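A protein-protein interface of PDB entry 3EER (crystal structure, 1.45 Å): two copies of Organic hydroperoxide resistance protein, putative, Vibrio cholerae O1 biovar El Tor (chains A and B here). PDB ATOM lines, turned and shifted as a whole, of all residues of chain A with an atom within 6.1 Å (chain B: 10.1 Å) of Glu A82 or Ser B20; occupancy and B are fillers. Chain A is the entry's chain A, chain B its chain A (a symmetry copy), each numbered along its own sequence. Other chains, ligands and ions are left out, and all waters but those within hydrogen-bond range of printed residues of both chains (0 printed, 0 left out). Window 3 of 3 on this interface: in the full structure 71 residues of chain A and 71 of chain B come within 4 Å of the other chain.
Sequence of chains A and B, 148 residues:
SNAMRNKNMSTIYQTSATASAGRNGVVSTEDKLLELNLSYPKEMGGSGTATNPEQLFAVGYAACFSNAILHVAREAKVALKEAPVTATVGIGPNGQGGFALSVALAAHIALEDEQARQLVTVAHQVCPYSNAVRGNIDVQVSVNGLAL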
ATOM      1  N   ALA A  62      27.180   6.951 -13.487  1.00  0.00           N
ATOM      2  CA  ALA A  62      27.647   7.421 -14.816  1.00  0.00           C
ATOM      3  C   ALA A  62      26.586   7.117 -15.890  1.00  0.00           C
ATOM      4  O   ALA A  62      26.186   7.994 -16.653  1.00  0.00           O
ATOM      5  CB  ALA A  62      28.975   6.818 -15.204  1.00  0.00           C
ATOM      6  N   SER A  66      24.283  10.045 -17.544  1.00  0.00           N
ATOM      7  CA  SER A  66      24.318  10.129 -18.989  1.00  0.00           C
ATOM      8  C   SER A  66      22.909   9.982 -19.564  1.00  0.00           C
ATOM      9  O   SER A  66      22.487  10.746 -20.451  1.00  0.00           O
ATOM     10  CB  SER A  66      25.254   9.046 -19.542  1.00  0.00           C
ATOM     11  OG  SER A  66      25.242   8.993 -20.977  1.00  0.00           O
ATOM     12  N   LEU A  70      20.477  12.602 -21.824  1.00  0.00           N
ATOM     13  CA  LEU A  70      19.832  12.166 -23.099  1.00  0.00           C
ATOM     14  C   LEU A  70      18.311  12.347 -23.036  1.00  0.00           C
ATOM     15  O   LEU A  70      17.687  12.781 -24.011  1.00  0.00           O
ATOM     16  CB  LEU A  70      20.242  10.731 -23.436  1.00  0.00           C
ATOM     17  CG  LEU A  70      21.709  10.518 -23.764  1.00  0.00           C
ATOM     18  CD1 LEU A  70      22.039   9.035 -23.902  1.00  0.00           C
ATOM     19  CD2 LEU A  70      22.142  11.267 -25.017  1.00  0.00           C
ATOM     20  N   LEU A  80      20.972  14.835 -29.555  1.00  0.00           N
ATOM     21  CA  LEU A  80      22.346  14.464 -29.079  1.00  0.00           C
ATOM     22  C   LEU A  80      22.742  13.075 -29.554  1.00  0.00           C
ATOM     23  O   LEU A  80      21.915  12.147 -29.486  1.00  0.00           O
ATOM     24  CB  LEU A  80      22.497  14.505 -27.552  1.00  0.00           C
ATOM     25  CG  LEU A  80      22.200  15.807 -26.804  1.00  0.00           C
ATOM     26  CD1 LEU A  80      22.483  15.569 -25.336  1.00  0.00           C
ATOM     27  CD2 LEU A  80      23.026  16.976 -27.366  1.00  0.00           C
ATOM     28  N   LYS A  81      23.982  12.917 -29.994  1.00  0.00           N
ATOM     29  CA  LYS A  81      24.504  11.614 -30.413  1.00  0.00           C
ATOM     30  C   LYS A  81      25.050  10.777 -29.251  1.00  0.00           C
ATOM     31  O   LYS A  81      25.092   9.538 -29.319  1.00  0.00           O
ATOM     32  CB  LYS A  81      25.642  11.829 -31.417  1.00  0.00           C
ATOM     33  CG  LYS A  81      25.214  12.492 -32.743  1.00  0.00           C
ATOM     34  CD  LYS A  81      26.075  12.056 -33.920  1.00  0.00           C
ATOM     35  CE  LYS A  81      25.529  12.580 -35.242  1.00  0.00           C
ATOM     36  NZ  LYS A  81      26.436  12.264 -36.406  1.00  0.00           N
ATOM     37  N   GLU A  82      25.488  11.460 -28.198  1.00  0.00           N
ATOM     38  CA  GLU A  82      26.141  10.814 -27.051  1.00  0.00           C
ATOM     39  C   GLU A  82      26.210  11.856 -25.938  1.00  0.00           C
ATOM     40  O   GLU A  82      26.106  13.035 -26.187  1.00  0.00           O
ATOM     41  CB  GLU A  82      27.558  10.296 -27.385  1.00  0.00           C
ATOM     42  CG  GLU A  82      28.538  11.344 -27.949  1.00  0.00           C
ATOM     43  CD  GLU A  82      29.779  10.719 -28.609  1.00  0.00           C
ATOM     44  OE1 GLU A  82      30.024   9.515 -28.363  1.00  0.00           O
ATOM     45  OE2 GLU A  82      30.509  11.431 -29.386  1.00  0.00           O
ATOM     46  N   ALA A  83      26.397  11.402 -24.711  1.00  0.00           N
ATOM     47  CA  ALA A  83      26.485  12.293 -23.562  1.00  0.00           C
ATOM     48  C   ALA A  83      27.459  11.665 -22.563  1.00  0.00           C
ATOM     49  O   ALA A  83      27.050  10.983 -21.597  1.00  0.00           O
ATOM     50  CB  ALA A  83      25.103  12.513 -22.911  1.00  0.00           C
ATOM     51  N   PRO A  84      28.766  11.830 -22.813  1.00  0.00           N
ATOM     52  CA  PRO A  84      29.778  11.217 -21.932  1.00  0.00           C
ATOM     53  C   PRO A  84      29.720  11.792 -20.525  1.00  0.00           C
ATOM     54  O   PRO A  84      29.795  13.018 -20.348  1.00  0.00           O
ATOM     55  CB  PRO A  84      31.117  11.553 -22.633  1.00  0.00           C
ATOM     56  CG  PRO A  84      30.728  11.854 -24.077  1.00  0.00           C
ATOM     57  CD  PRO A  84      29.380  12.507 -23.987  1.00  0.00           C
ATOM     58  N   VAL A  85      29.586  10.905 -19.537  1.00  0.00           N
ATOM     59  CA  VAL A  85      29.664  11.275 -18.140  1.00  0.00           C
ATOM     60  C   VAL A  85      30.673  10.381 -17.458  1.00  0.00           C
ATOM     61  O   VAL A  85      30.617   9.145 -17.614  1.00  0.00           O
ATOM     62  CB  VAL A  85      28.309  11.076 -17.440  1.00  0.00           C
ATOM     63  CG1 VAL A  85      28.467  11.298 -15.937  1.00  0.00           C
ATOM     64  CG2 VAL A  85      27.271  12.027 -18.070  1.00  0.00           C
ATOM     65  N   HIS A 108      29.508  15.921 -20.341  1.00  0.00           N
ATOM     66  CA  HIS A 108      29.962  16.479 -21.599  1.00  0.00           C
ATOM     67  C   HIS A 108      28.847  16.436 -22.617  1.00  0.00           C
ATOM     68  O   HIS A 108      28.220  15.395 -22.815  1.00  0.00           O
ATOM     69  CB  HIS A 108      31.181  15.688 -22.094  1.00  0.00           C
ATOM     70  CG  HIS A 108      32.246  15.564 -21.057  1.00  0.00           C
ATOM     71  ND1 HIS A 108      32.221  14.583 -20.087  1.00  0.00           N
ATOM     72  CD2 HIS A 108      33.363  16.302 -20.826  1.00  0.00           C
ATOM     73  CE1 HIS A 108      33.249  14.758 -19.275  1.00  0.00           C
ATOM     74  NE2 HIS A 108      33.968  15.791 -19.702  1.00  0.00           N
ATOM     75  N   ILE A 109      28.562  17.597 -23.204  1.00  0.00           N
ATOM     76  CA  ILE A 109      27.507  17.738 -24.230  1.00  0.00           C
ATOM     77  C   ILE A 109      28.084  18.587 -25.360  1.00  0.00           C
ATOM     78  O   ILE A 109      28.667  19.648 -25.119  1.00  0.00           O
ATOM     79  CB  ILE A 109      26.272  18.441 -23.647  1.00  0.00           C
ATOM     80  CG1 ILE A 109      25.688  17.631 -22.482  1.00  0.00           C
ATOM     81  CG2 ILE A 109      25.212  18.680 -24.727  1.00  0.00           C
ATOM     82  CD1 ILE A 109      24.513  18.320 -21.767  1.00  0.00           C
ATOM     83  N   ALA A 110      27.855  18.139 -26.600  1.00  0.00           N
ATOM     84  CA  ALA A 110      28.384  18.845 -27.797  1.00  0.00           C
ATOM     85  C   ALA A 110      27.491  20.005 -28.230  1.00  0.00           C
ATOM     86  O   ALA A 110      26.906  20.046 -29.320  1.00  0.00           O
ATOM     87  CB  ALA A 110      28.581  17.866 -28.940  1.00  0.00           C
ATOM     88  N   ALA B  17      34.163   5.833 -13.442  1.00  0.00           N
ATOM     89  CA  ALA B  17      33.575   5.093 -14.525  1.00  0.00           C
ATOM     90  C   ALA B  17      32.962   6.047 -15.514  1.00  0.00           C
ATOM     91  O   ALA B  17      32.536   7.146 -15.145  1.00  0.00           O
ATOM     92  CB  ALA B  17      32.504   4.177 -14.008  1.00  0.00           C
ATOM     93  N   THR B  18      32.855   5.613 -16.768  1.00  0.00           N
ATOM     94  CA  THR B  18      32.367   6.441 -17.865  1.00  0.00           C
ATOM     95  C   THR B  18      31.288   5.697 -18.672  1.00  0.00           C
ATOM     96  O   THR B  18      31.445   4.505 -19.003  1.00  0.00           O
ATOM     97  CB  THR B  18      33.503   6.894 -18.795  1.00  0.00           C
ATOM     98  OG1 THR B  18      34.474   7.629 -18.037  1.00  0.00           O
ATOM     99  CG2 THR B  18      32.958   7.767 -19.925  1.00  0.00           C
ATOM    100  N   ALA B  19      30.221   6.428 -18.967  1.00  0.00           N
ATOM    101  CA  ALA B  19      29.139   6.024 -19.845  1.00  0.00           C
ATOM    102  C   ALA B  19      28.812   7.161 -20.758  1.00  0.00           C
ATOM    103  O   ALA B  19      28.720   8.299 -20.287  1.00  0.00           O
ATOM    104  CB  ALA B  19      27.863   5.675 -19.050  1.00  0.00           C
ATOM    105  N   SER B  20      28.527   6.864 -22.022  1.00  0.00           N
ATOM    106  CA  SER B  20      28.142   7.912 -22.974  1.00  0.00           C
ATOM    107  C   SER B  20      26.831   7.674 -23.701  1.00  0.00           C
ATOM    108  O   SER B  20      26.359   8.565 -24.440  1.00  0.00           O
ATOM    109  CB  SER B  20      29.243   8.111 -24.006  1.00  0.00           C
ATOM    110  OG  SER B  20      30.501   8.266 -23.384  1.00  0.00           O
ATOM    111  N   ALA B  21      26.213   6.496 -23.503  1.00  0.00           N
ATOM    112  CA  ALA B  21      24.954   6.163 -24.167  1.00  0.00           C
ATOM    113  C   ALA B  21      23.860   5.863 -23.166  1.00  0.00           C
ATOM    114  O   ALA B  21      22.895   5.142 -23.458  1.00  0.00           O
ATOM    115  CB  ALA B  21      25.147   4.975 -25.116  1.00  0.00           C
ATOM    116  N   GLY B  22      23.974   6.439 -21.969  1.00  0.00           N
ATOM    117  CA  GLY B  22      22.951   6.243 -20.945  1.00  0.00           C
ATOM    118  C   GLY B  22      22.669   4.802 -20.644  1.00  0.00           C
ATOM    119  O   GLY B  22      23.570   3.972 -20.462  1.00  0.00           O
ATOM    120  N   ARG B  23      21.373   4.487 -20.596  1.00  0.00           N
ATOM    121  CA  ARG B  23      20.888   3.178 -20.201  1.00  0.00           C
ATOM    122  C   ARG B  23      20.932   2.141 -21.317  1.00  0.00           C
ATOM    123  O   ARG B  23      20.563   0.995 -21.110  1.00  0.00           O
ATOM    124  CB  ARG B  23      19.451   3.318 -19.663  1.00  0.00           C
ATOM    125  CG  ARG B  23      19.355   3.895 -18.278  1.00  0.00           C
ATOM    126  CD  ARG B  23      17.927   4.283 -17.933  1.00  0.00           C
ATOM    127  NE  ARG B  23      17.878   4.727 -16.560  1.00  0.00           N
ATOM    128  CZ  ARG B  23      17.535   3.994 -15.501  1.00  0.00           C
ATOM    129  NH1 ARG B  23      17.114   2.752 -15.628  1.00  0.00           N
ATOM    130  NH2 ARG B  23      17.600   4.523 -14.284  1.00  0.00           N
ATOM    131  N   ASN B  24      21.366   2.549 -22.504  1.00  0.00           N
ATOM    132  CA  ASN B  24      21.420   1.649 -23.661  1.00  0.00           C
ATOM    133  C   ASN B  24      22.749   1.695 -24.375  1.00  0.00           C
ATOM    134  O   ASN B  24      22.899   2.329 -25.382  1.00  0.00           O
ATOM    135  CB  ASN B  24      20.250   1.950 -24.579  1.00  0.00           C
ATOM    136  CG  ASN B  24      18.943   1.519 -23.961  1.00  0.00           C
ATOM    137  OD1 ASN B  24      18.581   0.326 -23.993  1.00  0.00           O
ATOM    138  ND2 ASN B  24      18.262   2.448 -23.300  1.00  0.00           N
ATOM    139  N   GLY B  25      23.739   1.059 -23.770  1.00  0.00           N
ATOM    140  CA  GLY B  25      25.109   1.144 -24.245  1.00  0.00           C
ATOM    141  C   GLY B  25      26.069   0.617 -23.198  1.00  0.00           C
ATOM    142  O   GLY B  25      25.672   0.077 -22.170  1.00  0.00           O
ATOM    143  N   VAL B  26      27.348   0.807 -23.439  1.00  0.00           N
ATOM    144  CA  VAL B  26      28.373   0.288 -22.557  1.00  0.00           C
ATOM    145  C   VAL B  26      28.684   1.268 -21.431  1.00  0.00           C
ATOM    146  O   VAL B  26      28.443   2.482 -21.507  1.00  0.00           O
ATOM    147  CB  VAL B  26      29.659  -0.075 -23.346  1.00  0.00           C
ATOM    148  CG1 VAL B  26      29.342  -1.143 -24.408  1.00  0.00           C
ATOM    149  CG2 VAL B  26      30.277   1.154 -23.981  1.00  0.00           C
ATOM    150  N   VAL B  27      29.221   0.715 -20.350  1.00  0.00           N
ATOM    151  CA  VAL B  27      29.776   1.495 -19.258  1.00  0.00           C
ATOM    152  C   VAL B  27      30.986   0.715 -18.707  1.00  0.00           C
ATOM    153  O   VAL B  27      31.010  -0.524 -18.711  1.00  0.00           O
ATOM    154  CB  VAL B  27      28.734   1.756 -18.144  1.00  0.00           C
ATOM    155  CG1 VAL B  27      28.208   0.433 -17.537  1.00  0.00           C
ATOM    156  CG2 VAL B  27      29.299   2.646 -17.025  1.00  0.00           C
ATOM    157  N   SER B  28      32.029   1.421 -18.267  1.00  0.00           N
ATOM    158  CA  SER B  28      33.180   0.722 -17.696  1.00  0.00           C
ATOM    159  C   SER B  28      33.869   1.571 -16.668  1.00  0.00           C
ATOM    160  O   SER B  28      33.819   2.809 -16.740  1.00  0.00           O
ATOM    161  CB  SER B  28      34.201   0.324 -18.766  1.00  0.00           C
ATOM    162  OG  SER B  28      34.642   1.441 -19.478  1.00  0.00           O
ATOM    163  N   LEU B  36      30.590  -3.372 -18.711  1.00  0.00           N
ATOM    164  CA  LEU B  36      29.260  -3.908 -18.837  1.00  0.00           C
ATOM    165  C   LEU B  36      28.556  -3.353 -20.044  1.00  0.00           C
ATOM    166  O   LEU B  36      28.735  -2.184 -20.431  1.00  0.00           O
ATOM    167  CB  LEU B  36      28.413  -3.567 -17.581  1.00  0.00           C
ATOM    168  CG  LEU B  36      28.897  -4.140 -16.251  1.00  0.00           C
ATOM    169  CD1 LEU B  36      28.141  -3.466 -15.083  1.00  0.00           C
ATOM    170  CD2 LEU B  36      28.762  -5.652 -16.201  1.00  0.00           C
ATOM    171  N   LEU B  38      24.640  -2.324 -20.964  1.00  0.00           N
ATOM    172  CA  LEU B  38      23.366  -1.973 -20.343  1.00  0.00           C
ATOM    173  C   LEU B  38      22.287  -1.935 -21.421  1.00  0.00           C
ATOM    174  O   LEU B  38      22.534  -1.444 -22.517  1.00  0.00           O
ATOM    175  CB  LEU B  38      23.404  -0.585 -19.698  1.00  0.00           C
ATOM    176  CG  LEU B  38      24.523  -0.341 -18.699  1.00  0.00           C
ATOM    177  CD1 LEU B  38      24.451   1.081 -18.155  1.00  0.00           C
ATOM    178  CD2 LEU B  38      24.530  -1.354 -17.566  1.00  0.00           C
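Of the 14 printed residues of chain B, 6 touch a printed residue of chain A. Printed residues of chain B that touch a printed residue of chain A: Ala B17, Thr B18, Ala B19, Ser B20, Ala B21 and Gly B22. Of the 12 printed residues of chain A, 7 touch a printed residue of chain B. Hydrophobic or aromatic side chains of chain A that line the printed part of chain B: Ala A62, Leu A70, Pro A84 and Val A85.
No position is printed for both chains. Of the 16 pairs that touch across the chains among the printed residues, none has its exchanged pair printed and touching as well.
N of Gly B22 lies within hydrogen-bond range of OG of Ser A66 (3.0 Å). O of Ser B20 is in hydrogen-bond range of N of Ala A83 (2.9 Å). The backbone carbonyl oxygen of Ala B19 is in hydrogen-bond range of the backbone NH of Val A85. O of Ala A83 sits close to O of Ala B19 (3.4 Å).
O of Ala A83 lies within hydrogen-bond range of OG of Ser A66 (2.8 Å). A ring nitrogen (ND1) of His A108 lies within hydrogen-bond range of the backbone carbonyl oxygen (O) of Pro A84, 2.9 Å away. The backbone NH of Thr B18 lies within hydrogen-bond range of the backbone carbonyl oxygen of Ser B28, 3.0 Å away.
Ala B17 touches Ala A62. Ala B19 touches Ala A62 (CB to C, 3.7 Å). OG of Ser A66 touches C of Ser B20 (3.4 Å). N of Ala B21 touches OG of Ser A66, at 3.7 Å. Leu A70 touches Ala B21 (CD1 to C, 3.7 Å). CD1 of Leu A70 touches N of Gly B22, 3.8 Å away. O of Ser B20 touches CA of Glu A82 (3.5 Å). Pro A84 touches Ala B19 (CA to O, 3.5 Å). O of Val A85 touches O of Ala B17, 3.7 Å away. Thr B18 touches Val A85.
Of the printed residues of chain B, Ala A62 touches Ala B17 and Ala B19. No residue of chain B comes within 4 Å of Leu A80. Of the printed residues of chain B, Glu A82 touches Ser B20. Of the printed residues of chain B, Pro A84 touches Ala B19 and Ser B20. Ala A110 touches none of the printed residues of chain B. Of the printed residues of chain A, Ala B17 touches Ala A62 and Val A85. Of the printed residues of chain A, Thr B18 touches Val A85. Asn B24 touches none of the printed residues of chain A. The nearest printed residue of chain B that does not touch Glu A82 is Ala B21 (5.6 Å). The nearest printed residue of chain A that does not touch Ser B20 is Leu A70 (4.4 Å). The nearest printed residue of chain A that does not touch Ala B17 is Pro A84 (7.6 Å).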
